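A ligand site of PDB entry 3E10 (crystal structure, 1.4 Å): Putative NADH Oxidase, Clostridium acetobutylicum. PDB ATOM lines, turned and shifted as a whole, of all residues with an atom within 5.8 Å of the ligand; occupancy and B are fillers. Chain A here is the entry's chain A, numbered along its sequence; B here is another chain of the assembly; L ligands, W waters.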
ATOM      1  N   ARG A   8       2.311 -31.303 -15.437  1.00  0.00           N
ATOM      2  CA  ARG A   8       2.443 -31.263 -13.987  1.00  0.00           C
ATOM      3  C   ARG A   8       1.103 -31.088 -13.313  1.00  0.00           C
ATOM      4  O   ARG A   8       0.375 -30.102 -13.588  1.00  0.00           O
ATOM      5  CB  ARG A   8       3.366 -30.121 -13.575  1.00  0.00           C
ATOM      6  CG  ARG A   8       3.517 -29.956 -12.064  1.00  0.00           C
ATOM      7  CD  ARG A   8       3.536 -28.481 -11.616  1.00  0.00           C
ATOM      8  NE  ARG A   8       2.351 -27.737 -12.043  1.00  0.00           N
ATOM      9  CZ  ARG A   8       1.158 -27.810 -11.438  1.00  0.00           C
ATOM     10  NH1 ARG A   8       0.969 -28.607 -10.400  1.00  0.00           N
ATOM     11  NH2 ARG A   8       0.148 -27.044 -11.909  1.00  0.00           N
ATOM     12  N   ARG A   9       0.758 -32.024 -12.419  1.00  0.00           N
ATOM     13  CA  ARG A   9      -0.501 -31.955 -11.652  1.00  0.00           C
ATOM     14  C   ARG A   9      -0.233 -32.132 -10.175  1.00  0.00           C
ATOM     15  O   ARG A   9       0.758 -32.773  -9.799  1.00  0.00           O
ATOM     16  CB  ARG A   9      -1.493 -33.054 -12.079  1.00  0.00           C
ATOM     17  CG  ARG A   9      -2.013 -32.931 -13.517  1.00  0.00           C
ATOM     18  CD  ARG A   9      -3.254 -32.034 -13.676  1.00  0.00           C
ATOM     19  NE  ARG A   9      -2.980 -30.610 -13.486  1.00  0.00           N
ATOM     20  CZ  ARG A   9      -2.427 -29.803 -14.399  1.00  0.00           C
ATOM     21  NH1 ARG A   9      -2.087 -30.228 -15.614  1.00  0.00           N
ATOM     22  NH2 ARG A   9      -2.223 -28.535 -14.093  1.00  0.00           N
ATOM     23  N   SER A  10      -1.118 -31.629  -9.332  1.00  0.00           N
ATOM     24  CA  SER A  10      -1.057 -31.950  -7.913  1.00  0.00           C
ATOM     25  C   SER A  10      -1.512 -33.387  -7.721  1.00  0.00           C
ATOM     26  O   SER A  10      -2.681 -33.668  -7.988  1.00  0.00           O
ATOM     27  CB  SER A  10      -1.915 -31.018  -7.076  1.00  0.00           C
ATOM     28  OG  SER A  10      -1.331 -29.724  -7.022  1.00  0.00           O
ATOM     29  N   ARG A  12      -1.718 -36.518  -4.958  1.00  0.00           N
ATOM     30  CA  ARG A  12      -1.869 -36.630  -3.526  1.00  0.00           C
ATOM     31  C   ARG A  12      -2.001 -38.082  -3.026  1.00  0.00           C
ATOM     32  O   ARG A  12      -2.320 -38.305  -1.870  1.00  0.00           O
ATOM     33  CB  ARG A  12      -3.097 -35.847  -3.071  1.00  0.00           C
ATOM     34  CG  ARG A  12      -3.058 -34.350  -3.475  1.00  0.00           C
ATOM     35  CD  ARG A  12      -4.272 -33.593  -2.910  1.00  0.00           C
ATOM     36  NE  ARG A  12      -4.171 -32.169  -3.175  1.00  0.00           N
ATOM     37  CZ  ARG A  12      -4.480 -31.593  -4.319  1.00  0.00           C
ATOM     38  NH1 ARG A  12      -4.959 -32.276  -5.344  1.00  0.00           N
ATOM     39  NH2 ARG A  12      -4.347 -30.264  -4.438  1.00  0.00           N
ATOM     40  N   SER A  61      -0.960 -29.331   8.987  1.00  0.00           N
ATOM     41  CA  SER A  61      -2.086 -28.564   8.476  1.00  0.00           C
ATOM     42  C   SER A  61      -3.235 -29.530   8.230  1.00  0.00           C
ATOM     43  O   SER A  61      -3.035 -30.750   8.238  1.00  0.00           O
ATOM     44  CB  SER A  61      -1.720 -27.763   7.237  1.00  0.00           C
ATOM     45  OG  SER A  61      -2.133 -28.347   6.050  1.00  0.00           O
ATOM     46  N   TYR A  63      -4.734 -29.690   5.391  1.00  0.00           N
ATOM     47  CA  TYR A  63      -4.721 -29.960   3.961  1.00  0.00           C
ATOM     48  C   TYR A  63      -3.489 -30.756   3.509  1.00  0.00           C
ATOM     49  O   TYR A  63      -3.055 -30.652   2.375  1.00  0.00           O
ATOM     50  CB  TYR A  63      -4.825 -28.640   3.218  1.00  0.00           C
ATOM     51  CG  TYR A  63      -6.071 -27.924   3.598  1.00  0.00           C
ATOM     52  CD1 TYR A  63      -7.271 -28.220   2.987  1.00  0.00           C
ATOM     53  CD2 TYR A  63      -6.053 -26.965   4.604  1.00  0.00           C
ATOM     54  CE1 TYR A  63      -8.455 -27.553   3.369  1.00  0.00           C
ATOM     55  CE2 TYR A  63      -7.213 -26.284   4.975  1.00  0.00           C
ATOM     56  CZ  TYR A  63      -8.395 -26.598   4.362  1.00  0.00           C
ATOM     57  OH  TYR A  63      -9.542 -25.945   4.731  1.00  0.00           O
ATOM     58  N   ALA A  64      -2.993 -31.598   4.403  1.00  0.00           N
ATOM     59  CA  ALA A  64      -1.734 -32.295   4.199  1.00  0.00           C
ATOM     60  C   ALA A  64      -1.874 -33.824   4.278  1.00  0.00           C
ATOM     61  O   ALA A  64      -0.909 -34.538   4.565  1.00  0.00           O
ATOM     62  CB  ALA A  64      -0.667 -31.772   5.215  1.00  0.00           C
ATOM     63  N   VAL A 112       2.752 -32.792  -4.648  1.00  0.00           N
ATOM     64  CA  VAL A 112       1.876 -31.675  -4.375  1.00  0.00           C
ATOM     65  C   VAL A 112       2.550 -30.737  -3.394  1.00  0.00           C
ATOM     66  O   VAL A 112       3.183 -31.157  -2.415  1.00  0.00           O
ATOM     67  CB  VAL A 112       0.490 -32.155  -3.806  1.00  0.00           C
ATOM     68  CG1 VAL A 112       0.645 -32.989  -2.516  1.00  0.00           C
ATOM     69  CG2 VAL A 112      -0.497 -30.968  -3.607  1.00  0.00           C
ATOM     70  N   TRP A 113       2.346 -29.459  -3.656  1.00  0.00           N
ATOM     71  CA  TRP A 113       2.775 -28.367  -2.767  1.00  0.00           C
ATOM     72  C   TRP A 113       1.758 -28.219  -1.660  1.00  0.00           C
ATOM     73  O   TRP A 113       0.548 -27.990  -1.916  1.00  0.00           O
ATOM     74  CB  TRP A 113       2.794 -27.101  -3.623  1.00  0.00           C
ATOM     75  CG  TRP A 113       3.194 -25.792  -3.022  1.00  0.00           C
ATOM     76  CD1 TRP A 113       3.110 -25.347  -1.728  1.00  0.00           C
ATOM     77  CD2 TRP A 113       3.701 -24.705  -3.792  1.00  0.00           C
ATOM     78  NE1 TRP A 113       3.533 -24.031  -1.658  1.00  0.00           N
ATOM     79  CE2 TRP A 113       3.934 -23.629  -2.904  1.00  0.00           C
ATOM     80  CE3 TRP A 113       4.022 -24.547  -5.147  1.00  0.00           C
ATOM     81  CZ2 TRP A 113       4.413 -22.411  -3.344  1.00  0.00           C
ATOM     82  CZ3 TRP A 113       4.504 -23.346  -5.562  1.00  0.00           C
ATOM     83  CH2 TRP A 113       4.687 -22.283  -4.667  1.00  0.00           C
ATOM     84  N   LEU A 114       2.233 -28.321  -0.417  1.00  0.00           N
ATOM     85  CA  LEU A 114       1.417 -28.194   0.764  1.00  0.00           C
ATOM     86  C   LEU A 114       1.773 -26.885   1.468  1.00  0.00           C
ATOM     87  O   LEU A 114       2.846 -26.761   2.053  1.00  0.00           O
ATOM     88  CB  LEU A 114       1.584 -29.409   1.694  1.00  0.00           C
ATOM     89  CG  LEU A 114       1.365 -30.761   1.021  1.00  0.00           C
ATOM     90  CD1 LEU A 114       1.768 -31.880   2.026  1.00  0.00           C
ATOM     91  CD2 LEU A 114      -0.076 -30.941   0.525  1.00  0.00           C
ATOM     92  N   GLY A 115       0.910 -25.898   1.324  1.00  0.00           N
ATOM     93  CA  GLY A 115       1.204 -24.531   1.787  1.00  0.00           C
ATOM     94  C   GLY A 115       1.411 -24.475   3.277  1.00  0.00           C
ATOM     95  O   GLY A 115       0.749 -25.184   4.025  1.00  0.00           O
ATOM     96  N   ARG A 122       0.314 -23.244  10.907  1.00  0.00           N
ATOM     97  CA  ARG A 122       1.139 -24.173  10.132  1.00  0.00           C
ATOM     98  C   ARG A 122       2.644 -23.936  10.342  1.00  0.00           C
ATOM     99  O   ARG A 122       3.416 -24.900  10.515  1.00  0.00           O
ATOM    100  CB  ARG A 122       0.815 -24.047   8.640  1.00  0.00           C
ATOM    101  CG  ARG A 122      -0.647 -24.355   8.355  1.00  0.00           C
ATOM    102  CD  ARG A 122      -0.917 -24.343   6.885  1.00  0.00           C
ATOM    103  NE  ARG A 122      -2.337 -24.357   6.641  1.00  0.00           N
ATOM    104  CZ  ARG A 122      -2.880 -24.311   5.444  1.00  0.00           C
ATOM    105  NH1 ARG A 122      -2.133 -24.305   4.356  1.00  0.00           N
ATOM    106  NH2 ARG A 122      -4.190 -24.273   5.325  1.00  0.00           N
ATOM    107  N   ILE A 155      -4.424 -30.564 -18.062  1.00  0.00           N
ATOM    108  CA  ILE A 155      -5.672 -29.855 -17.887  1.00  0.00           C
ATOM    109  C   ILE A 155      -5.412 -28.455 -18.464  1.00  0.00           C
ATOM    110  O   ILE A 155      -4.534 -27.748 -17.975  1.00  0.00           O
ATOM    111  CB  ILE A 155      -6.089 -29.711 -16.393  1.00  0.00           C
ATOM    112  CG1 ILE A 155      -6.300 -31.086 -15.769  1.00  0.00           C
ATOM    113  CG2 ILE A 155      -7.333 -28.843 -16.257  1.00  0.00           C
ATOM    114  CD1 ILE A 155      -6.464 -31.058 -14.226  1.00  0.00           C
ATOM    115  N   ARG A 157      -5.694 -24.844 -18.722  1.00  0.00           N
ATOM    116  CA  ARG A 157      -6.136 -23.788 -17.840  1.00  0.00           C
ATOM    117  C   ARG A 157      -6.103 -22.420 -18.558  1.00  0.00           C
ATOM    118  O   ARG A 157      -6.394 -21.379 -17.959  1.00  0.00           O
ATOM    119  CB  ARG A 157      -5.207 -23.726 -16.625  1.00  0.00           C
ATOM    120  CG  ARG A 157      -5.222 -24.971 -15.711  1.00  0.00           C
ATOM    121  CD  ARG A 157      -6.192 -24.749 -14.571  1.00  0.00           C
ATOM    122  NE  ARG A 157      -6.416 -25.959 -13.792  1.00  0.00           N
ATOM    123  CZ  ARG A 157      -5.545 -26.481 -12.930  1.00  0.00           C
ATOM    124  NH1 ARG A 157      -4.359 -25.920 -12.725  1.00  0.00           N
ATOM    125  NH2 ARG A 157      -5.850 -27.597 -12.301  1.00  0.00           N
ATOM    126  N   GLN B  33      -0.642 -22.476 -16.484  1.00  0.00           N
ATOM    127  CA  GLN B  33      -0.562 -23.842 -15.989  1.00  0.00           C
ATOM    128  C   GLN B  33       0.047 -23.962 -14.595  1.00  0.00           C
ATOM    129  O   GLN B  33       0.170 -25.065 -14.068  1.00  0.00           O
ATOM    130  CB  GLN B  33       0.239 -24.715 -16.961  1.00  0.00           C
ATOM    131  CG  GLN B  33      -0.406 -24.932 -18.290  1.00  0.00           C
ATOM    132  CD  GLN B  33      -1.777 -25.539 -18.229  1.00  0.00           C
ATOM    133  OE1 GLN B  33      -2.755 -24.948 -18.720  1.00  0.00           O
ATOM    134  NE2 GLN B  33      -1.897 -26.711 -17.600  1.00  0.00           N
ATOM    135  N   ALA B  34       0.407 -22.849 -13.971  1.00  0.00           N
ATOM    136  CA  ALA B  34       0.987 -22.901 -12.641  1.00  0.00           C
ATOM    137  C   ALA B  34       0.007 -23.419 -11.594  1.00  0.00           C
ATOM    138  O   ALA B  34      -1.222 -23.259 -11.722  1.00  0.00           O
ATOM    139  CB  ALA B  34       1.506 -21.530 -12.240  1.00  0.00           C
ATOM    140  N   PRO B  35       0.561 -24.046 -10.556  1.00  0.00           N
ATOM    141  CA  PRO B  35      -0.275 -24.375  -9.431  1.00  0.00           C
ATOM    142  C   PRO B  35      -0.703 -23.083  -8.735  1.00  0.00           C
ATOM    143  O   PRO B  35      -0.068 -22.037  -8.892  1.00  0.00           O
ATOM    144  CB  PRO B  35       0.643 -25.208  -8.540  1.00  0.00           C
ATOM    145  CG  PRO B  35       1.988 -24.641  -8.817  1.00  0.00           C
ATOM    146  CD  PRO B  35       1.982 -24.373 -10.318  1.00  0.00           C
ATOM    147  N   SER B  36      -1.781 -23.149  -7.945  1.00  0.00           N
ATOM    148  CA  SER B  36      -2.225 -21.997  -7.171  1.00  0.00           C
ATOM    149  C   SER B  36      -3.014 -22.455  -5.981  1.00  0.00           C
ATOM    150  O   SER B  36      -3.712 -23.469  -6.042  1.00  0.00           O
ATOM    151  CB  SER B  36      -3.013 -20.994  -8.024  1.00  0.00           C
ATOM    152  OG  SER B  36      -4.231 -21.505  -8.555  1.00  0.00           O
ATOM    153  N   ALA B  37      -2.856 -21.749  -4.878  1.00  0.00           N
ATOM    154  CA  ALA B  37      -3.551 -22.114  -3.631  1.00  0.00           C
ATOM    155  C   ALA B  37      -5.044 -22.139  -3.890  1.00  0.00           C
ATOM    156  O   ALA B  37      -5.616 -21.199  -4.466  1.00  0.00           O
ATOM    157  CB  ALA B  37      -3.189 -21.145  -2.512  1.00  0.00           C
ATOM    158  N   GLY B  38      -5.698 -23.230  -3.492  1.00  0.00           N
ATOM    159  CA  GLY B  38      -7.140 -23.321  -3.744  1.00  0.00           C
ATOM    160  C   GLY B  38      -7.553 -23.392  -5.217  1.00  0.00           C
ATOM    161  O   GLY B  38      -8.704 -23.197  -5.543  1.00  0.00           O
ATOM    162  N   ASN B  39      -6.593 -23.628  -6.124  1.00  0.00           N
ATOM    163  CA  ASN B  39      -6.800 -23.465  -7.545  1.00  0.00           C
ATOM    164  C   ASN B  39      -7.426 -22.093  -7.888  1.00  0.00           C
ATOM    165  O   ASN B  39      -8.233 -21.981  -8.820  1.00  0.00           O
ATOM    166  CB  ASN B  39      -7.705 -24.579  -8.096  1.00  0.00           C
ATOM    167  CG  ASN B  39      -7.685 -24.684  -9.610  1.00  0.00           C
ATOM    168  OD1 ASN B  39      -6.684 -24.387 -10.271  1.00  0.00           O
ATOM    169  ND2 ASN B  39      -8.824 -25.089 -10.183  1.00  0.00           N
ATOM    170  N   MET B  88      -1.797 -16.447   0.196  1.00  0.00           N
ATOM    171  CA  MET B  88      -0.765 -17.107  -0.606  1.00  0.00           C
ATOM    172  C   MET B  88      -0.656 -16.601  -2.046  1.00  0.00           C
ATOM    173  O   MET B  88       0.036 -17.206  -2.839  1.00  0.00           O
ATOM    174  CB  MET B  88      -0.947 -18.621  -0.572  1.00  0.00           C
ATOM    175  CG  MET B  88      -0.502 -19.230   0.747  1.00  0.00           C
ATOM    176  SD  MET B  88      -1.147 -21.020   0.968  1.00  0.00           S
ATOM    177  CE  MET B  88      -0.732 -21.184   2.828  1.00  0.00           C
ATOM    178  N   GLN B  91       2.723 -16.431  -3.842  1.00  0.00           N
ATOM    179  CA  GLN B  91       3.311 -17.724  -4.169  1.00  0.00           C
ATOM    180  C   GLN B  91       2.775 -18.244  -5.482  1.00  0.00           C
ATOM    181  O   GLN B  91       3.546 -18.730  -6.330  1.00  0.00           O
ATOM    182  CB  GLN B  91       3.052 -18.708  -3.024  1.00  0.00           C
ATOM    183  CG  GLN B  91       3.711 -18.241  -1.711  1.00  0.00           C
ATOM    184  CD  GLN B  91       3.411 -19.138  -0.523  1.00  0.00           C
ATOM    185  OE1 GLN B  91       3.254 -20.353  -0.683  1.00  0.00           O
ATOM    186  NE2 GLN B  91       3.303 -18.532   0.671  1.00  0.00           N
ATOM    187  N   ASP B  92       1.472 -18.142  -5.669  1.00  0.00           N
ATOM    188  CA  ASP B  92       0.857 -18.494  -6.930  1.00  0.00           C
ATOM    189  C   ASP B  92       1.542 -17.744  -8.088  1.00  0.00           C
ATOM    190  O   ASP B  92       1.823 -18.308  -9.124  1.00  0.00           O
ATOM    191  CB  ASP B  92      -0.612 -18.063  -6.960  1.00  0.00           C
ATOM    192  CG  ASP B  92      -1.488 -18.682  -5.899  1.00  0.00           C
ATOM    193  OD1 ASP B  92      -1.050 -19.639  -5.212  1.00  0.00           O
ATOM    194  OD2 ASP B  92      -2.662 -18.210  -5.809  1.00  0.00           O
ATOM    195  N   ALA B  95       5.010 -18.858  -8.878  1.00  0.00           N
ATOM    196  CA  ALA B  95       5.021 -20.126  -9.638  1.00  0.00           C
ATOM    197  C   ALA B  95       4.731 -19.851 -11.120  1.00  0.00           C
ATOM    198  O   ALA B  95       5.354 -20.457 -11.995  1.00  0.00           O
ATOM    199  CB  ALA B  95       3.982 -21.093  -9.020  1.00  0.00           C
HETATM  200  N1  LIG L   1      -2.822 -28.650  -2.223  1.00  0.00           N
HETATM  201  C1  LIG L   1      -3.188 -29.313  -1.081  1.00  0.00           C
HETATM  202  O1  LIG L   1      -3.712 -30.433  -1.147  1.00  0.00           O
HETATM  203  N2  LIG L   1      -2.926 -28.786   0.165  1.00  0.00           N
HETATM  204  C2  LIG L   1      -2.398 -27.531   0.328  1.00  0.00           C
HETATM  205  O2  LIG L   1      -2.136 -27.108   1.477  1.00  0.00           O
HETATM  206  C3  LIG L   1      -1.994 -26.847  -0.840  1.00  0.00           C
HETATM  207  N3  LIG L   1      -1.391 -25.622  -0.750  1.00  0.00           N
HETATM  208  C4  LIG L   1      -0.981 -24.958  -1.879  1.00  0.00           C
HETATM  209  C5  LIG L   1      -0.346 -23.714  -1.784  1.00  0.00           C
HETATM  210  C6  LIG L   1       0.098 -23.026  -2.885  1.00  0.00           C
HETATM  211  C7  LIG L   1       0.785 -21.697  -2.710  1.00  0.00           C
HETATM  212  C8  LIG L   1      -0.076 -23.598  -4.150  1.00  0.00           C
HETATM  213  C9  LIG L   1       0.627 -22.964  -5.315  1.00  0.00           C
HETATM  214  C10 LIG L   1      -0.702 -24.842  -4.263  1.00  0.00           C
HETATM  215  C11 LIG L   1      -1.155 -25.530  -3.145  1.00  0.00           C
HETATM  216  N4  LIG L   1      -1.835 -26.752  -3.253  1.00  0.00           N
HETATM  217  C12 LIG L   1      -2.209 -27.423  -2.104  1.00  0.00           C
HETATM  218  C13 LIG L   1      -2.073 -27.382  -4.595  1.00  0.00           C
HETATM  219  C14 LIG L   1      -3.258 -26.698  -5.303  1.00  0.00           C
HETATM  220  O3  LIG L   1      -4.499 -27.078  -4.720  1.00  0.00           O
HETATM  221  C15 LIG L   1      -3.217 -27.016  -6.784  1.00  0.00           C
HETATM  222  O4  LIG L   1      -2.038 -26.416  -7.344  1.00  0.00           O
HETATM  223  C16 LIG L   1      -4.469 -26.533  -7.563  1.00  0.00           C
HETATM  224  O5  LIG L   1      -5.633 -27.212  -7.151  1.00  0.00           O
HETATM  225  C17 LIG L   1      -4.294 -26.684  -9.061  1.00  0.00           C
HETATM  226  O6  LIG L   1      -4.160 -28.051  -9.433  1.00  0.00           O
HETATM  227  P1  LIG L   1      -2.826 -28.505 -10.199  1.00  0.00           P
HETATM  228  O7  LIG L   1      -1.665 -28.355  -9.227  1.00  0.00           O
HETATM  229  O8  LIG L   1      -3.077 -29.964 -10.555  1.00  0.00           O
HETATM  230  O9  LIG L   1      -2.653 -27.643 -11.441  1.00  0.00           O
HETATM  231  O   HOH W   1      -8.464 -27.203  -5.130  1.00  0.00           O
HETATM  232  O   HOH W   2      -5.582 -31.672   0.460  1.00  0.00           O
HETATM  233  O   HOH W   3      -0.879 -27.551   3.889  1.00  0.00           O
HETATM  234  O   HOH W   4      -5.531 -29.958  -7.246  1.00  0.00           O
HETATM  235  O   HOH W   5      -3.921 -23.557 -10.273  1.00  0.00           O
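Water W4 bridges O5 of the ligand (2.7 Å) and NH1 of Arg 12 (3.1 Å). Water W3 lies within hydrogen-bond range of the side-chain hydroxyl (OG) of Ser 61 (2.6 Å), an oxygen (O2) of the ligand (2.8 Å) and the backbone carbonyl oxygen (O) of Gly 115 (2.9 Å). Water W2 lies within hydrogen-bond range of an oxygen (O1) of the ligand and the backbone carbonyl oxygen (O) of Tyr 63. Water W5 lies within hydrogen-bond range of the side-chain hydroxyl of Ser 36 of chain B, the side-chain amide oxygen of Asn 39 of chain B, the backbone carbonyl oxygen of Ala 34 of chain B and the guanidinium group of Arg 157.
O of Trp 113 lies close to N4 of the ligand (3.0 Å). Val 112 touches the ligand. CD2 of Leu 114 touches N2 of the ligand, at 3.6 Å. Pro 35 of chain B touches the ligand. Ala 37 of chain B touches the ligand (N to C8, 3.4 Å). CB of Asn 39 of chain B touches O5 of the ligand, at 3.5 Å. SD of Met 88 of chain B touches C5 of the ligand, at 3.9 Å. Gln 91 of chain B touches the ligand (OE1 to C7, 3.5 Å). Asp 92 of chain B touches the ligand (OD1 to C7, 3.7 Å).
The backbone NH (N) of Arg 157 sits at hydrogen-bond distance from the side-chain amide oxygen (OE1) of Gln 33 of chain B (2.9 Å). The side-chain hydroxyl (OG) of Ser 61 is in hydrogen-bond range of the backbone NH (N) of Tyr 63. The guanidinium group (NH2) of Arg 8 sits at hydrogen-bond distance from the backbone carbonyl oxygen (O) of Gln 33 of chain B (2.9 Å). The guanidinium group of Arg 122 is in hydrogen-bond range of the backbone carbonyl oxygen of Gly 115 (3.0 Å). N of Ala 37 of chain B is in hydrogen-bond range of OD1 of Asp 92 of chain B, at 2.8 Å.
An oxygen (O8) of the ligand lies within hydrogen-bond range of the backbone NH of Ser 10 (2.8 Å). The side-chain hydroxyl (OG) of Ser 10 lies within hydrogen-bond range of an oxygen (O7) of the ligand, at 2.6 Å. The guanidinium group of Arg 12 lies within hydrogen-bond range of an oxygen (O1) of the ligand (2.7 Å). NH1 of Arg 157 is in salt-bridge range of O9 of the ligand (2.7 Å). NH2 of Arg 9 lies within salt-bridge range of O9 of the ligand, 2.8 Å away. A nitrogen (N2) of the ligand lies within hydrogen-bond range of the backbone carbonyl oxygen (O) of Tyr 63 (2.9 Å). NH1 of Arg 8 lies within salt-bridge range of O7 of the ligand, 2.9 Å away. N of Gly 115 lies within hydrogen-bond range of N3 of the ligand (3.1 Å). An oxygen (O4) of the ligand is in hydrogen-bond range of the backbone NH (N) of Ser 36 of chain B, 3.3 Å away.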
